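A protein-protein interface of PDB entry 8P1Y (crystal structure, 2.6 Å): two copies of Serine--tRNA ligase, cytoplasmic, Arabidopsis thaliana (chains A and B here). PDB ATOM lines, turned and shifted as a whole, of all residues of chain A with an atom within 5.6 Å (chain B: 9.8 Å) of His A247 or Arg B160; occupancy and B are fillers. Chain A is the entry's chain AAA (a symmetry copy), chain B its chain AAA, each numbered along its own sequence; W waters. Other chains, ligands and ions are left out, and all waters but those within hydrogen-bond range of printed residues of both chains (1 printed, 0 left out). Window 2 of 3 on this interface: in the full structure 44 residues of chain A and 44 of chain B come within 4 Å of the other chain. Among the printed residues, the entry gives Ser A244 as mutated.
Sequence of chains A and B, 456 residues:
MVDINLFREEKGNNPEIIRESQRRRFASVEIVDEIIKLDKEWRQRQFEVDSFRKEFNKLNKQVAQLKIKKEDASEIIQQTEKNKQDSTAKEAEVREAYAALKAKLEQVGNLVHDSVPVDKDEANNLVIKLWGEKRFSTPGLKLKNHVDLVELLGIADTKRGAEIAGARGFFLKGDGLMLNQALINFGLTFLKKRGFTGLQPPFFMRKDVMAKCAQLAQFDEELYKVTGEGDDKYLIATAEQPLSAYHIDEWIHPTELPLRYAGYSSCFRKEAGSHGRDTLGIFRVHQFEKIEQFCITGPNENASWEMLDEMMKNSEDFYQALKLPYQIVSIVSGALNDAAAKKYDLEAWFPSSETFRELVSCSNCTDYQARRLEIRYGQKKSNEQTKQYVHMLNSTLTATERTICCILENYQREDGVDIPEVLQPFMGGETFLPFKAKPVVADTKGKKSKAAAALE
The side-chain carboxylate of Asp B157 sits at hydrogen-bond distance from the side-chain hydroxyl of Tyr A246 (3.0 Å). The guanidinium group (NH1) of Arg B160 sits at hydrogen-bond distance from the side-chain hydroxyl (OH) of Tyr A246 (3.0 Å). OE1 of Glu A250 is in salt-bridge range of NE of Arg B160, 2.6 Å away. The side-chain hydroxyl (OH) of Tyr A246 is in hydrogen-bond range of the side-chain amino group (NZ) of Lys B173 (3.3 Å).
The side-chain carboxylate (OD1) of Asp B157 lies within hydrogen-bond range of the backbone NH (N) of Lys B159 (3.2 Å). The side-chain carboxylate (OD2) of Asp B157 is in salt-bridge range of the guanidinium group (NH1) of Arg B160 (3.1 Å). The backbone NH of Asp B157 lies within hydrogen-bond range of the backbone carbonyl oxygen of Phe B171 (3.0 Å). A ring nitrogen (ND1) of His A247 sits at hydrogen-bond distance from the side-chain carboxylate (OE2) of Glu A250 (3.0 Å). NE2 of His A247 is in hydrogen-bond range of OH of Tyr A261.
Among the printed residues, pairs that only touch across the chains: Ala A245 with Ile B164, Tyr A246 with Phe B171 and His A247 with Arg B160.
His A247 touches one residue of chain B. Arg B160 touches three residues of chain A. Of chain B, only Asp B157, Arg B160, Phe B171 and Lys B173 come within 4 Å of Tyr A246. Printed residues of chain A within 4 Å of Ile B164: Ala A245 (3.5 Å). Printed residues of chain B within 4 Å of Ala A245: Ile B164. Of the printed residues of chain A, Asp B157 touches Tyr A246 (3.0 Å). Of the printed residues of chain A, Lys B173 touches Tyr A246. Leu B280 touches none of the printed residues of chain A. The nearest residue of chain B that does not touch His A247 is Lys B173 (6.0 Å). The nearest printed residue of chain A that does not touch Arg B160 is Tyr A261 (5.9 Å).
Of the 17 printed residues of chain A, 4 touch a printed residue of chain B. Along chain A the printed residues that touch a printed residue of chain B span positions 245 to 250. Printed residues of chain B that touch a printed residue of chain A: Asp B157, Arg B160, Ile B164, Phe B171 and Lys B173.
No position is printed for both chains. Of the 7 pairs that touch across the chains among the printed residues, none has its exchanged pair printed and touching as well.
Water W1 bridges the side-chain hydroxyl of Tyr A261 (2.8 Å) and the side-chain amino group of Lys B173 (3.0 Å).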
ATOM      1  N   LEU A 243     -14.558  13.586   7.764  1.00  0.00           N
ATOM      2  CA  LEU A 243     -15.655  14.345   7.119  1.00  0.00           C
ATOM      3  C   LEU A 243     -15.791  13.890   5.661  1.00  0.00           C
ATOM      4  O   LEU A 243     -16.939  13.820   5.159  1.00  0.00           O
ATOM      5  CB  LEU A 243     -15.349  15.839   7.240  1.00  0.00           C
ATOM      6  CG  LEU A 243     -15.895  16.522   8.494  1.00  0.00           C
ATOM      7  CD1 LEU A 243     -15.329  15.926   9.763  1.00  0.00           C
ATOM      8  CD2 LEU A 243     -15.624  18.011   8.462  1.00  0.00           C
ATOM      9  N   SER A 244     -14.664  13.565   5.025  1.00  0.00           N
ATOM     10  CA  SER A 244     -14.604  12.988   3.658  1.00  0.00           C
ATOM     11  C   SER A 244     -15.371  11.661   3.626  1.00  0.00           C
ATOM     12  O   SER A 244     -16.112  11.439   2.641  1.00  0.00           O
ATOM     13  CB  SER A 244     -13.187  12.788   3.226  1.00  0.00           C
ATOM     14  OG  SER A 244     -12.612  11.712   3.953  1.00  0.00           O
ATOM     15  N   ALA A 245     -15.198  10.827   4.665  1.00  0.00           N
ATOM     16  CA  ALA A 245     -15.836   9.494   4.814  1.00  0.00           C
ATOM     17  C   ALA A 245     -17.345   9.617   5.095  1.00  0.00           C
ATOM     18  O   ALA A 245     -18.100   8.724   4.644  1.00  0.00           O
ATOM     19  CB  ALA A 245     -15.142   8.702   5.887  1.00  0.00           C
ATOM     20  N   TYR A 246     -17.800  10.654   5.806  1.00  0.00           N
ATOM     21  CA  TYR A 246     -19.245  11.017   5.842  1.00  0.00           C
ATOM     22  C   TYR A 246     -19.705  11.117   4.381  1.00  0.00           C
ATOM     23  O   TYR A 246     -18.984  11.776   3.589  1.00  0.00           O
ATOM     24  CB  TYR A 246     -19.458  12.348   6.574  1.00  0.00           C
ATOM     25  CG  TYR A 246     -20.787  12.571   7.261  1.00  0.00           C
ATOM     26  CD1 TYR A 246     -20.988  12.160   8.572  1.00  0.00           C
ATOM     27  CD2 TYR A 246     -21.809  13.291   6.653  1.00  0.00           C
ATOM     28  CE1 TYR A 246     -22.180  12.403   9.237  1.00  0.00           C
ATOM     29  CE2 TYR A 246     -23.008  13.544   7.303  1.00  0.00           C
ATOM     30  CZ  TYR A 246     -23.196  13.096   8.601  1.00  0.00           C
ATOM     31  OH  TYR A 246     -24.375  13.326   9.251  1.00  0.00           O
ATOM     32  N   HIS A 247     -20.822  10.481   4.023  1.00  0.00           N
ATOM     33  CA  HIS A 247     -21.405  10.492   2.647  1.00  0.00           C
ATOM     34  C   HIS A 247     -20.686   9.525   1.690  1.00  0.00           C
ATOM     35  O   HIS A 247     -21.025   9.573   0.489  1.00  0.00           O
ATOM     36  CB  HIS A 247     -21.449  11.900   2.026  1.00  0.00           C
ATOM     37  CG  HIS A 247     -22.379  12.849   2.706  1.00  0.00           C
ATOM     38  ND1 HIS A 247     -23.694  12.526   2.993  1.00  0.00           N
ATOM     39  CD2 HIS A 247     -22.195  14.120   3.132  1.00  0.00           C
ATOM     40  CE1 HIS A 247     -24.275  13.547   3.591  1.00  0.00           C
ATOM     41  NE2 HIS A 247     -23.374  14.542   3.685  1.00  0.00           N
ATOM     42  N   ILE A 248     -19.782   8.668   2.185  1.00  0.00           N
ATOM     43  CA  ILE A 248     -19.197   7.500   1.452  1.00  0.00           C
ATOM     44  C   ILE A 248     -20.306   6.549   0.958  1.00  0.00           C
ATOM     45  O   ILE A 248     -21.264   6.284   1.714  1.00  0.00           O
ATOM     46  CB  ILE A 248     -18.187   6.742   2.336  1.00  0.00           C
ATOM     47  CG1 ILE A 248     -17.436   5.662   1.553  1.00  0.00           C
ATOM     48  CG2 ILE A 248     -18.876   6.160   3.554  1.00  0.00           C
ATOM     49  CD1 ILE A 248     -16.645   4.692   2.414  1.00  0.00           C
ATOM     50  N   ASP A 249     -20.170   6.047  -0.275  1.00  0.00           N
ATOM     51  CA  ASP A 249     -21.127   5.136  -0.962  1.00  0.00           C
ATOM     52  C   ASP A 249     -22.529   5.737  -1.050  1.00  0.00           C
ATOM     53  O   ASP A 249     -23.427   4.988  -1.443  1.00  0.00           O
ATOM     54  CB  ASP A 249     -21.258   3.792  -0.254  1.00  0.00           C
ATOM     55  CG  ASP A 249     -19.972   2.995  -0.246  1.00  0.00           C
ATOM     56  OD1 ASP A 249     -19.281   2.992  -1.280  1.00  0.00           O
ATOM     57  OD2 ASP A 249     -19.663   2.395   0.802  1.00  0.00           O
ATOM     58  N   GLU A 250     -22.714   7.022  -0.729  1.00  0.00           N
ATOM     59  CA  GLU A 250     -24.032   7.701  -0.789  1.00  0.00           C
ATOM     60  C   GLU A 250     -24.233   8.367  -2.152  1.00  0.00           C
ATOM     61  O   GLU A 250     -23.247   8.608  -2.872  1.00  0.00           O
ATOM     62  CB  GLU A 250     -24.152   8.754   0.307  1.00  0.00           C
ATOM     63  CG  GLU A 250     -23.845   8.222   1.691  1.00  0.00           C
ATOM     64  CD  GLU A 250     -24.417   9.076   2.809  1.00  0.00           C
ATOM     65  OE1 GLU A 250     -24.030   8.864   3.974  1.00  0.00           O
ATOM     66  OE2 GLU A 250     -25.237   9.967   2.509  1.00  0.00           O
ATOM     67  N   TRP A 251     -25.494   8.630  -2.481  1.00  0.00           N
ATOM     68  CA  TRP A 251     -25.937   9.553  -3.557  1.00  0.00           C
ATOM     69  C   TRP A 251     -26.283  10.892  -2.900  1.00  0.00           C
ATOM     70  O   TRP A 251     -26.789  10.870  -1.748  1.00  0.00           O
ATOM     71  CB  TRP A 251     -27.137   8.966  -4.314  1.00  0.00           C
ATOM     72  CG  TRP A 251     -26.767   7.874  -5.268  1.00  0.00           C
ATOM     73  CD1 TRP A 251     -26.361   6.608  -4.957  1.00  0.00           C
ATOM     74  CD2 TRP A 251     -26.758   7.957  -6.705  1.00  0.00           C
ATOM     75  NE1 TRP A 251     -26.099   5.899  -6.096  1.00  0.00           N
ATOM     76  CE2 TRP A 251     -26.329   6.700  -7.185  1.00  0.00           C
ATOM     77  CE3 TRP A 251     -27.074   8.962  -7.627  1.00  0.00           C
ATOM     78  CZ2 TRP A 251     -26.207   6.425  -8.548  1.00  0.00           C
ATOM     79  CZ3 TRP A 251     -26.953   8.690  -8.972  1.00  0.00           C
ATOM     80  CH2 TRP A 251     -26.525   7.438  -9.425  1.00  0.00           C
ATOM     81  N   ILE A 252     -25.981  12.014  -3.559  1.00  0.00           N
ATOM     82  CA  ILE A 252     -26.378  13.363  -3.064  1.00  0.00           C
ATOM     83  C   ILE A 252     -27.104  14.077  -4.210  1.00  0.00           C
ATOM     84  O   ILE A 252     -26.674  13.940  -5.374  1.00  0.00           O
ATOM     85  CB  ILE A 252     -25.195  14.155  -2.442  1.00  0.00           C
ATOM     86  CG1 ILE A 252     -24.078  14.444  -3.437  1.00  0.00           C
ATOM     87  CG2 ILE A 252     -24.612  13.473  -1.202  1.00  0.00           C
ATOM     88  CD1 ILE A 252     -22.913  15.145  -2.767  1.00  0.00           C
ATOM     89  N   LEU A 259     -23.052  21.733   0.258  1.00  0.00           N
ATOM     90  CA  LEU A 259     -22.997  21.337   1.684  1.00  0.00           C
ATOM     91  C   LEU A 259     -21.809  22.037   2.367  1.00  0.00           C
ATOM     92  O   LEU A 259     -20.730  22.199   1.750  1.00  0.00           O
ATOM     93  CB  LEU A 259     -22.912  19.809   1.777  1.00  0.00           C
ATOM     94  CG  LEU A 259     -24.198  19.048   1.442  1.00  0.00           C
ATOM     95  CD1 LEU A 259     -23.982  17.544   1.515  1.00  0.00           C
ATOM     96  CD2 LEU A 259     -25.337  19.468   2.363  1.00  0.00           C
ATOM     97  N   TYR A 261     -19.914  21.964   6.051  1.00  0.00           N
ATOM     98  CA  TYR A 261     -19.598  21.405   7.380  1.00  0.00           C
ATOM     99  C   TYR A 261     -18.439  22.198   8.001  1.00  0.00           C
ATOM    100  O   TYR A 261     -17.314  22.289   7.449  1.00  0.00           O
ATOM    101  CB  TYR A 261     -19.331  19.910   7.225  1.00  0.00           C
ATOM    102  CG  TYR A 261     -20.451  19.138   6.574  1.00  0.00           C
ATOM    103  CD1 TYR A 261     -21.701  19.077   7.154  1.00  0.00           C
ATOM    104  CD2 TYR A 261     -20.255  18.439   5.401  1.00  0.00           C
ATOM    105  CE1 TYR A 261     -22.726  18.345   6.584  1.00  0.00           C
ATOM    106  CE2 TYR A 261     -21.269  17.707   4.810  1.00  0.00           C
ATOM    107  CZ  TYR A 261     -22.514  17.655   5.405  1.00  0.00           C
ATOM    108  OH  TYR A 261     -23.532  16.941   4.832  1.00  0.00           O
ATOM    109  N   ILE A 296     -18.935  20.399  -0.172  1.00  0.00           N
ATOM    110  CA  ILE A 296     -19.276  19.501  -1.312  1.00  0.00           C
ATOM    111  C   ILE A 296     -20.103  20.315  -2.296  1.00  0.00           C
ATOM    112  O   ILE A 296     -20.976  21.040  -1.831  1.00  0.00           O
ATOM    113  CB  ILE A 296     -20.026  18.247  -0.829  1.00  0.00           C
ATOM    114  CG1 ILE A 296     -19.233  17.502   0.250  1.00  0.00           C
ATOM    115  CG2 ILE A 296     -20.350  17.355  -2.013  1.00  0.00           C
ATOM    116  CD1 ILE A 296     -19.931  16.287   0.827  1.00  0.00           C
ATOM    117  N   LEU A 373     -14.313   7.260  -2.753  1.00  0.00           N
ATOM    118  CA  LEU A 373     -15.355   7.037  -1.704  1.00  0.00           C
ATOM    119  C   LEU A 373     -16.738   6.807  -2.348  1.00  0.00           C
ATOM    120  O   LEU A 373     -17.742   6.900  -1.632  1.00  0.00           O
ATOM    121  CB  LEU A 373     -15.385   8.240  -0.748  1.00  0.00           C
ATOM    122  CG  LEU A 373     -14.077   8.594  -0.040  1.00  0.00           C
ATOM    123  CD1 LEU A 373     -14.303   9.647   1.031  1.00  0.00           C
ATOM    124  CD2 LEU A 373     -13.437   7.374   0.587  1.00  0.00           C
ATOM    125  N   GLU A 374     -16.807   6.525  -3.648  1.00  0.00           N
ATOM    126  CA  GLU A 374     -18.075   6.312  -4.399  1.00  0.00           C
ATOM    127  C   GLU A 374     -19.174   7.263  -3.905  1.00  0.00           C
ATOM    128  O   GLU A 374     -20.263   6.784  -3.571  1.00  0.00           O
ATOM    129  CB  GLU A 374     -18.480   4.843  -4.293  1.00  0.00           C
ATOM    130  CG  GLU A 374     -17.952   3.997  -5.434  1.00  0.00           C
ATOM    131  CD  GLU A 374     -18.389   4.483  -6.808  1.00  0.00           C
ATOM    132  OE1 GLU A 374     -19.597   4.826  -6.959  1.00  0.00           O
ATOM    133  OE2 GLU A 374     -17.518   4.545  -7.715  1.00  0.00           O
ATOM    134  N   ILE A 375     -18.895   8.569  -3.896  1.00  0.00           N
ATOM    135  CA  ILE A 375     -19.838   9.655  -3.488  1.00  0.00           C
ATOM    136  C   ILE A 375     -20.417  10.308  -4.749  1.00  0.00           C
ATOM    137  O   ILE A 375     -19.789  11.261  -5.271  1.00  0.00           O
ATOM    138  CB  ILE A 375     -19.137  10.686  -2.588  1.00  0.00           C
ATOM    139  CG1 ILE A 375     -18.384  10.014  -1.443  1.00  0.00           C
ATOM    140  CG2 ILE A 375     -20.130  11.697  -2.070  1.00  0.00           C
ATOM    141  CD1 ILE A 375     -17.711  10.975  -0.473  1.00  0.00           C
ATOM    142  N   MET A 392     -15.236  18.083  -3.795  1.00  0.00           N
ATOM    143  CA  MET A 392     -15.029  18.326  -2.349  1.00  0.00           C
ATOM    144  C   MET A 392     -13.807  19.209  -2.163  1.00  0.00           C
ATOM    145  O   MET A 392     -12.809  18.933  -2.777  1.00  0.00           O
ATOM    146  CB  MET A 392     -14.832  17.033  -1.560  1.00  0.00           C
ATOM    147  CG  MET A 392     -15.788  15.919  -1.954  1.00  0.00           C
ATOM    148  SD  MET A 392     -15.588  14.465  -0.883  1.00  0.00           S
ATOM    149  CE  MET A 392     -17.055  14.675   0.111  1.00  0.00           C
ATOM    150  N   GLY B 154     -31.791  15.206  15.052  1.00  0.00           N
ATOM    151  CA  GLY B 154     -30.764  15.313  13.995  1.00  0.00           C
ATOM    152  C   GLY B 154     -29.459  15.912  14.508  1.00  0.00           C
ATOM    153  O   GLY B 154     -28.859  16.731  13.766  1.00  0.00           O
ATOM    154  N   ALA B 156     -26.875  13.944  16.183  1.00  0.00           N
ATOM    155  CA  ALA B 156     -25.792  12.939  16.140  1.00  0.00           C
ATOM    156  C   ALA B 156     -26.005  12.064  14.911  1.00  0.00           C
ATOM    157  O   ALA B 156     -27.167  11.922  14.511  1.00  0.00           O
ATOM    158  CB  ALA B 156     -25.766  12.120  17.404  1.00  0.00           C
ATOM    159  N   ASP B 157     -24.922  11.580  14.300  1.00  0.00           N
ATOM    160  CA  ASP B 157     -24.995  10.549  13.238  1.00  0.00           C
ATOM    161  C   ASP B 157     -24.180   9.352  13.692  1.00  0.00           C
ATOM    162  O   ASP B 157     -22.958   9.348  13.509  1.00  0.00           O
ATOM    163  CB  ASP B 157     -24.570  11.028  11.856  1.00  0.00           C
ATOM    164  CG  ASP B 157     -25.239  10.164  10.803  1.00  0.00           C
ATOM    165  OD1 ASP B 157     -25.266   8.919  10.993  1.00  0.00           O
ATOM    166  OD2 ASP B 157     -25.794  10.736   9.850  1.00  0.00           O
ATOM    167  N   THR B 158     -24.880   8.399  14.293  1.00  0.00           N
ATOM    168  CA  THR B 158     -24.323   7.187  14.928  1.00  0.00           C
ATOM    169  C   THR B 158     -24.152   6.134  13.829  1.00  0.00           C
ATOM    170  O   THR B 158     -23.273   5.265  13.997  1.00  0.00           O
ATOM    171  CB  THR B 158     -25.210   6.789  16.118  1.00  0.00           C
ATOM    172  OG1 THR B 158     -26.547   6.545  15.669  1.00  0.00           O
ATOM    173  CG2 THR B 158     -25.233   7.860  17.189  1.00  0.00           C
ATOM    174  N   LYS B 159     -24.946   6.231  12.753  1.00  0.00           N
ATOM    175  CA  LYS B 159     -24.884   5.311  11.583  1.00  0.00           C
ATOM    176  C   LYS B 159     -23.574   5.563  10.828  1.00  0.00           C
ATOM    177  O   LYS B 159     -22.727   4.651  10.774  1.00  0.00           O
ATOM    178  CB  LYS B 159     -26.088   5.500  10.648  1.00  0.00           C
ATOM    179  CG  LYS B 159     -27.270   4.560  10.875  1.00  0.00           C
ATOM    180  CD  LYS B 159     -28.582   5.091  10.295  1.00  0.00           C
ATOM    181  CE  LYS B 159     -29.335   4.097   9.431  1.00  0.00           C
ATOM    182  NZ  LYS B 159     -30.064   3.089  10.238  1.00  0.00           N
ATOM    183  N   ARG B 160     -23.419   6.764  10.267  1.00  0.00           N
ATOM    184  CA  ARG B 160     -22.200   7.177   9.522  1.00  0.00           C
ATOM    185  C   ARG B 160     -21.012   7.151  10.508  1.00  0.00           C
ATOM    186  O   ARG B 160     -19.888   6.807  10.093  1.00  0.00           O
ATOM    187  CB  ARG B 160     -22.435   8.524   8.822  1.00  0.00           C
ATOM    188  CG  ARG B 160     -23.473   8.514   7.697  1.00  0.00           C
ATOM    189  CD  ARG B 160     -23.851   9.936   7.282  1.00  0.00           C
ATOM    190  NE  ARG B 160     -24.795  10.135   6.168  1.00  0.00           N
ATOM    191  CZ  ARG B 160     -25.715  11.119   6.084  1.00  0.00           C
ATOM    192  NH1 ARG B 160     -25.868  11.991   7.065  1.00  0.00           N
ATOM    193  NH2 ARG B 160     -26.506  11.223   5.028  1.00  0.00           N
ATOM    194  N   GLY B 161     -21.250   7.433  11.789  1.00  0.00           N
ATOM    195  CA  GLY B 161     -20.211   7.389  12.838  1.00  0.00           C
ATOM    196  C   GLY B 161     -19.647   5.990  13.015  1.00  0.00           C
ATOM    197  O   GLY B 161     -18.426   5.882  13.253  1.00  0.00           O
ATOM    198  N   ALA B 162     -20.503   4.964  12.890  1.00  0.00           N
ATOM    199  CA  ALA B 162     -20.202   3.535  13.169  1.00  0.00           C
ATOM    200  C   ALA B 162     -19.382   2.920  12.032  1.00  0.00           C
ATOM    201  O   ALA B 162     -18.472   2.130  12.337  1.00  0.00           O
ATOM    202  CB  ALA B 162     -21.478   2.760  13.379  1.00  0.00           C
ATOM    203  N   GLU B 163     -19.721   3.259  10.783  1.00  0.00           N
ATOM    204  CA  GLU B 163     -18.976   2.872   9.551  1.00  0.00           C
ATOM    205  C   GLU B 163     -17.583   3.515   9.506  1.00  0.00           C
ATOM    206  O   GLU B 163     -16.758   2.978   8.748  1.00  0.00           O
ATOM    207  CB  GLU B 163     -19.741   3.288   8.294  1.00  0.00           C
ATOM    208  CG  GLU B 163     -20.894   2.368   7.956  1.00  0.00           C
ATOM    209  CD  GLU B 163     -21.808   2.927   6.883  1.00  0.00           C
ATOM    210  OE1 GLU B 163     -21.321   3.734   6.058  1.00  0.00           O
ATOM    211  OE2 GLU B 163     -23.001   2.565   6.882  1.00  0.00           O
ATOM    212  N   ILE B 164     -17.335   4.616  10.241  1.00  0.00           N
ATOM    213  CA  ILE B 164     -16.037   5.377  10.237  1.00  0.00           C
ATOM    214  C   ILE B 164     -15.132   4.876  11.382  1.00  0.00           C
ATOM    215  O   ILE B 164     -14.015   4.420  11.077  1.00  0.00           O
ATOM    216  CB  ILE B 164     -16.259   6.916  10.266  1.00  0.00           C
ATOM    217  CG1 ILE B 164     -16.527   7.504   8.875  1.00  0.00           C
ATOM    218  CG2 ILE B 164     -15.091   7.652  10.919  1.00  0.00           C
ATOM    219  CD1 ILE B 164     -17.614   6.809   8.078  1.00  0.00           C
ATOM    220  N   ALA B 165     -15.576   4.950  12.642  1.00  0.00           N
ATOM    221  CA  ALA B 165     -14.744   4.684  13.843  1.00  0.00           C
ATOM    222  C   ALA B 165     -15.049   3.299  14.415  1.00  0.00           C
ATOM    223  O   ALA B 165     -14.469   2.961  15.472  1.00  0.00           O
ATOM    224  CB  ALA B 165     -14.983   5.743  14.888  1.00  0.00           C
ATOM    225  N   GLY B 166     -15.919   2.533  13.749  1.00  0.00           N
ATOM    226  CA  GLY B 166     -16.422   1.248  14.258  1.00  0.00           C
ATOM    227  C   GLY B 166     -17.480   1.478  15.319  1.00  0.00           C
ATOM    228  O   GLY B 166     -17.941   2.633  15.438  1.00  0.00           O
ATOM    229  N   ALA B 167     -17.790   0.440  16.103  1.00  0.00           N
ATOM    230  CA  ALA B 167     -19.021   0.301  16.920  1.00  0.00           C
ATOM    231  C   ALA B 167     -19.026   1.288  18.095  1.00  0.00           C
ATOM    232  O   ALA B 167     -18.008   1.365  18.826  1.00  0.00           O
ATOM    233  CB  ALA B 167     -19.161  -1.129  17.398  1.00  0.00           C
ATOM    234  N   ARG B 168     -20.166   1.971  18.266  1.00  0.00           N
ATOM    235  CA  ARG B 168     -20.488   2.966  19.333  1.00  0.00           C
ATOM    236  C   ARG B 168     -19.793   4.291  19.001  1.00  0.00           C
ATOM    237  O   ARG B 168     -19.592   5.116  19.926  1.00  0.00           O
ATOM    238  CB  ARG B 168     -20.164   2.416  20.727  1.00  0.00           C
ATOM    239  CG  ARG B 168     -21.006   1.211  21.125  1.00  0.00           C
ATOM    240  CD  ARG B 168     -22.456   1.554  21.443  1.00  0.00           C
ATOM    241  NE  ARG B 168     -23.192   0.426  22.015  1.00  0.00           N
ATOM    242  CZ  ARG B 168     -22.984  -0.123  23.224  1.00  0.00           C
ATOM    243  NH1 ARG B 168     -23.728  -1.144  23.619  1.00  0.00           N
ATOM    244  NH2 ARG B 168     -22.038   0.331  24.036  1.00  0.00           N
ATOM    245  N   GLY B 169     -19.496   4.485  17.708  1.00  0.00           N
ATOM    246  CA  GLY B 169     -18.891   5.700  17.132  1.00  0.00           C
ATOM    247  C   GLY B 169     -19.952   6.645  16.598  1.00  0.00           C
ATOM    248  O   GLY B 169     -20.843   6.191  15.847  1.00  0.00           O
ATOM    249  N   PHE B 170     -19.851   7.924  16.963  1.00  0.00           N
ATOM    250  CA  PHE B 170     -20.857   8.974  16.652  1.00  0.00           C
ATOM    251  C   PHE B 170     -20.151  10.244  16.144  1.00  0.00           C
ATOM    252  O   PHE B 170     -19.016  10.563  16.600  1.00  0.00           O
ATOM    253  CB  PHE B 170     -21.722   9.223  17.894  1.00  0.00           C
ATOM    254  CG  PHE B 170     -20.976   9.684  19.127  1.00  0.00           C
ATOM    255  CD1 PHE B 170     -20.436   8.777  20.031  1.00  0.00           C
ATOM    256  CD2 PHE B 170     -20.819  11.031  19.402  1.00  0.00           C
ATOM    257  CE1 PHE B 170     -19.759   9.209  21.168  1.00  0.00           C
ATOM    258  CE2 PHE B 170     -20.136  11.458  20.533  1.00  0.00           C
ATOM    259  CZ  PHE B 170     -19.615  10.549  21.421  1.00  0.00           C
ATOM    260  N   PHE B 171     -20.804  10.941  15.211  1.00  0.00           N
ATOM    261  CA  PHE B 171     -20.649  12.402  14.994  1.00  0.00           C
ATOM    262  C   PHE B 171     -21.629  13.151  15.913  1.00  0.00           C
ATOM    263  O   PHE B 171     -22.787  12.748  15.988  1.00  0.00           O
ATOM    264  CB  PHE B 171     -20.921  12.772  13.531  1.00  0.00           C
ATOM    265  CG  PHE B 171     -19.912  12.249  12.539  1.00  0.00           C
ATOM    266  CD1 PHE B 171     -19.987  10.946  12.072  1.00  0.00           C
ATOM    267  CD2 PHE B 171     -18.890  13.055  12.067  1.00  0.00           C
ATOM    268  CE1 PHE B 171     -19.063  10.461  11.159  1.00  0.00           C
ATOM    269  CE2 PHE B 171     -17.972  12.568  11.152  1.00  0.00           C
ATOM    270  CZ  PHE B 171     -18.056  11.272  10.703  1.00  0.00           C
ATOM    271  N   LEU B 172     -21.192  14.210  16.599  1.00  0.00           N
ATOM    272  CA  LEU B 172     -22.103  15.322  16.994  1.00  0.00           C
ATOM    273  C   LEU B 172     -22.389  16.181  15.753  1.00  0.00           C
ATOM    274  O   LEU B 172     -21.553  16.234  14.847  1.00  0.00           O
ATOM    275  CB  LEU B 172     -21.464  16.158  18.102  1.00  0.00           C
ATOM    276  CG  LEU B 172     -21.366  15.475  19.460  1.00  0.00           C
ATOM    277  CD1 LEU B 172     -20.693  16.398  20.474  1.00  0.00           C
ATOM    278  CD2 LEU B 172     -22.741  15.040  19.946  1.00  0.00           C
ATOM    279  N   LYS B 173     -23.545  16.819  15.688  1.00  0.00           N
ATOM    280  CA  LYS B 173     -23.950  17.561  14.476  1.00  0.00           C
ATOM    281  C   LYS B 173     -24.818  18.748  14.888  1.00  0.00           C
ATOM    282  O   LYS B 173     -25.464  18.665  15.948  1.00  0.00           O
ATOM    283  CB  LYS B 173     -24.630  16.594  13.506  1.00  0.00           C
ATOM    284  CG  LYS B 173     -25.257  17.259  12.298  1.00  0.00           C
ATOM    285  CD  LYS B 173     -25.627  16.291  11.213  1.00  0.00           C
ATOM    286  CE  LYS B 173     -25.846  16.999   9.895  1.00  0.00           C
ATOM    287  NZ  LYS B 173     -26.186  16.041   8.822  1.00  0.00           N
ATOM    288  N   LEU B 280     -28.761   2.705  18.364  1.00  0.00           N
ATOM    289  CA  LEU B 280     -27.463   3.417  18.508  1.00  0.00           C
ATOM    290  C   LEU B 280     -27.730   4.775  19.185  1.00  0.00           C
ATOM    291  O   LEU B 280     -28.517   5.563  18.607  1.00  0.00           O
ATOM    292  CB  LEU B 280     -26.815   3.562  17.120  1.00  0.00           C
ATOM    293  CG  LEU B 280     -26.671   2.281  16.281  1.00  0.00           C
ATOM    294  CD1 LEU B 280     -26.108   2.585  14.892  1.00  0.00           C
ATOM    295  CD2 LEU B 280     -25.807   1.240  16.988  1.00  0.00           C
HETATM  296  O   HOH W   1     -26.028  17.297   6.149  1.00  0.00           O
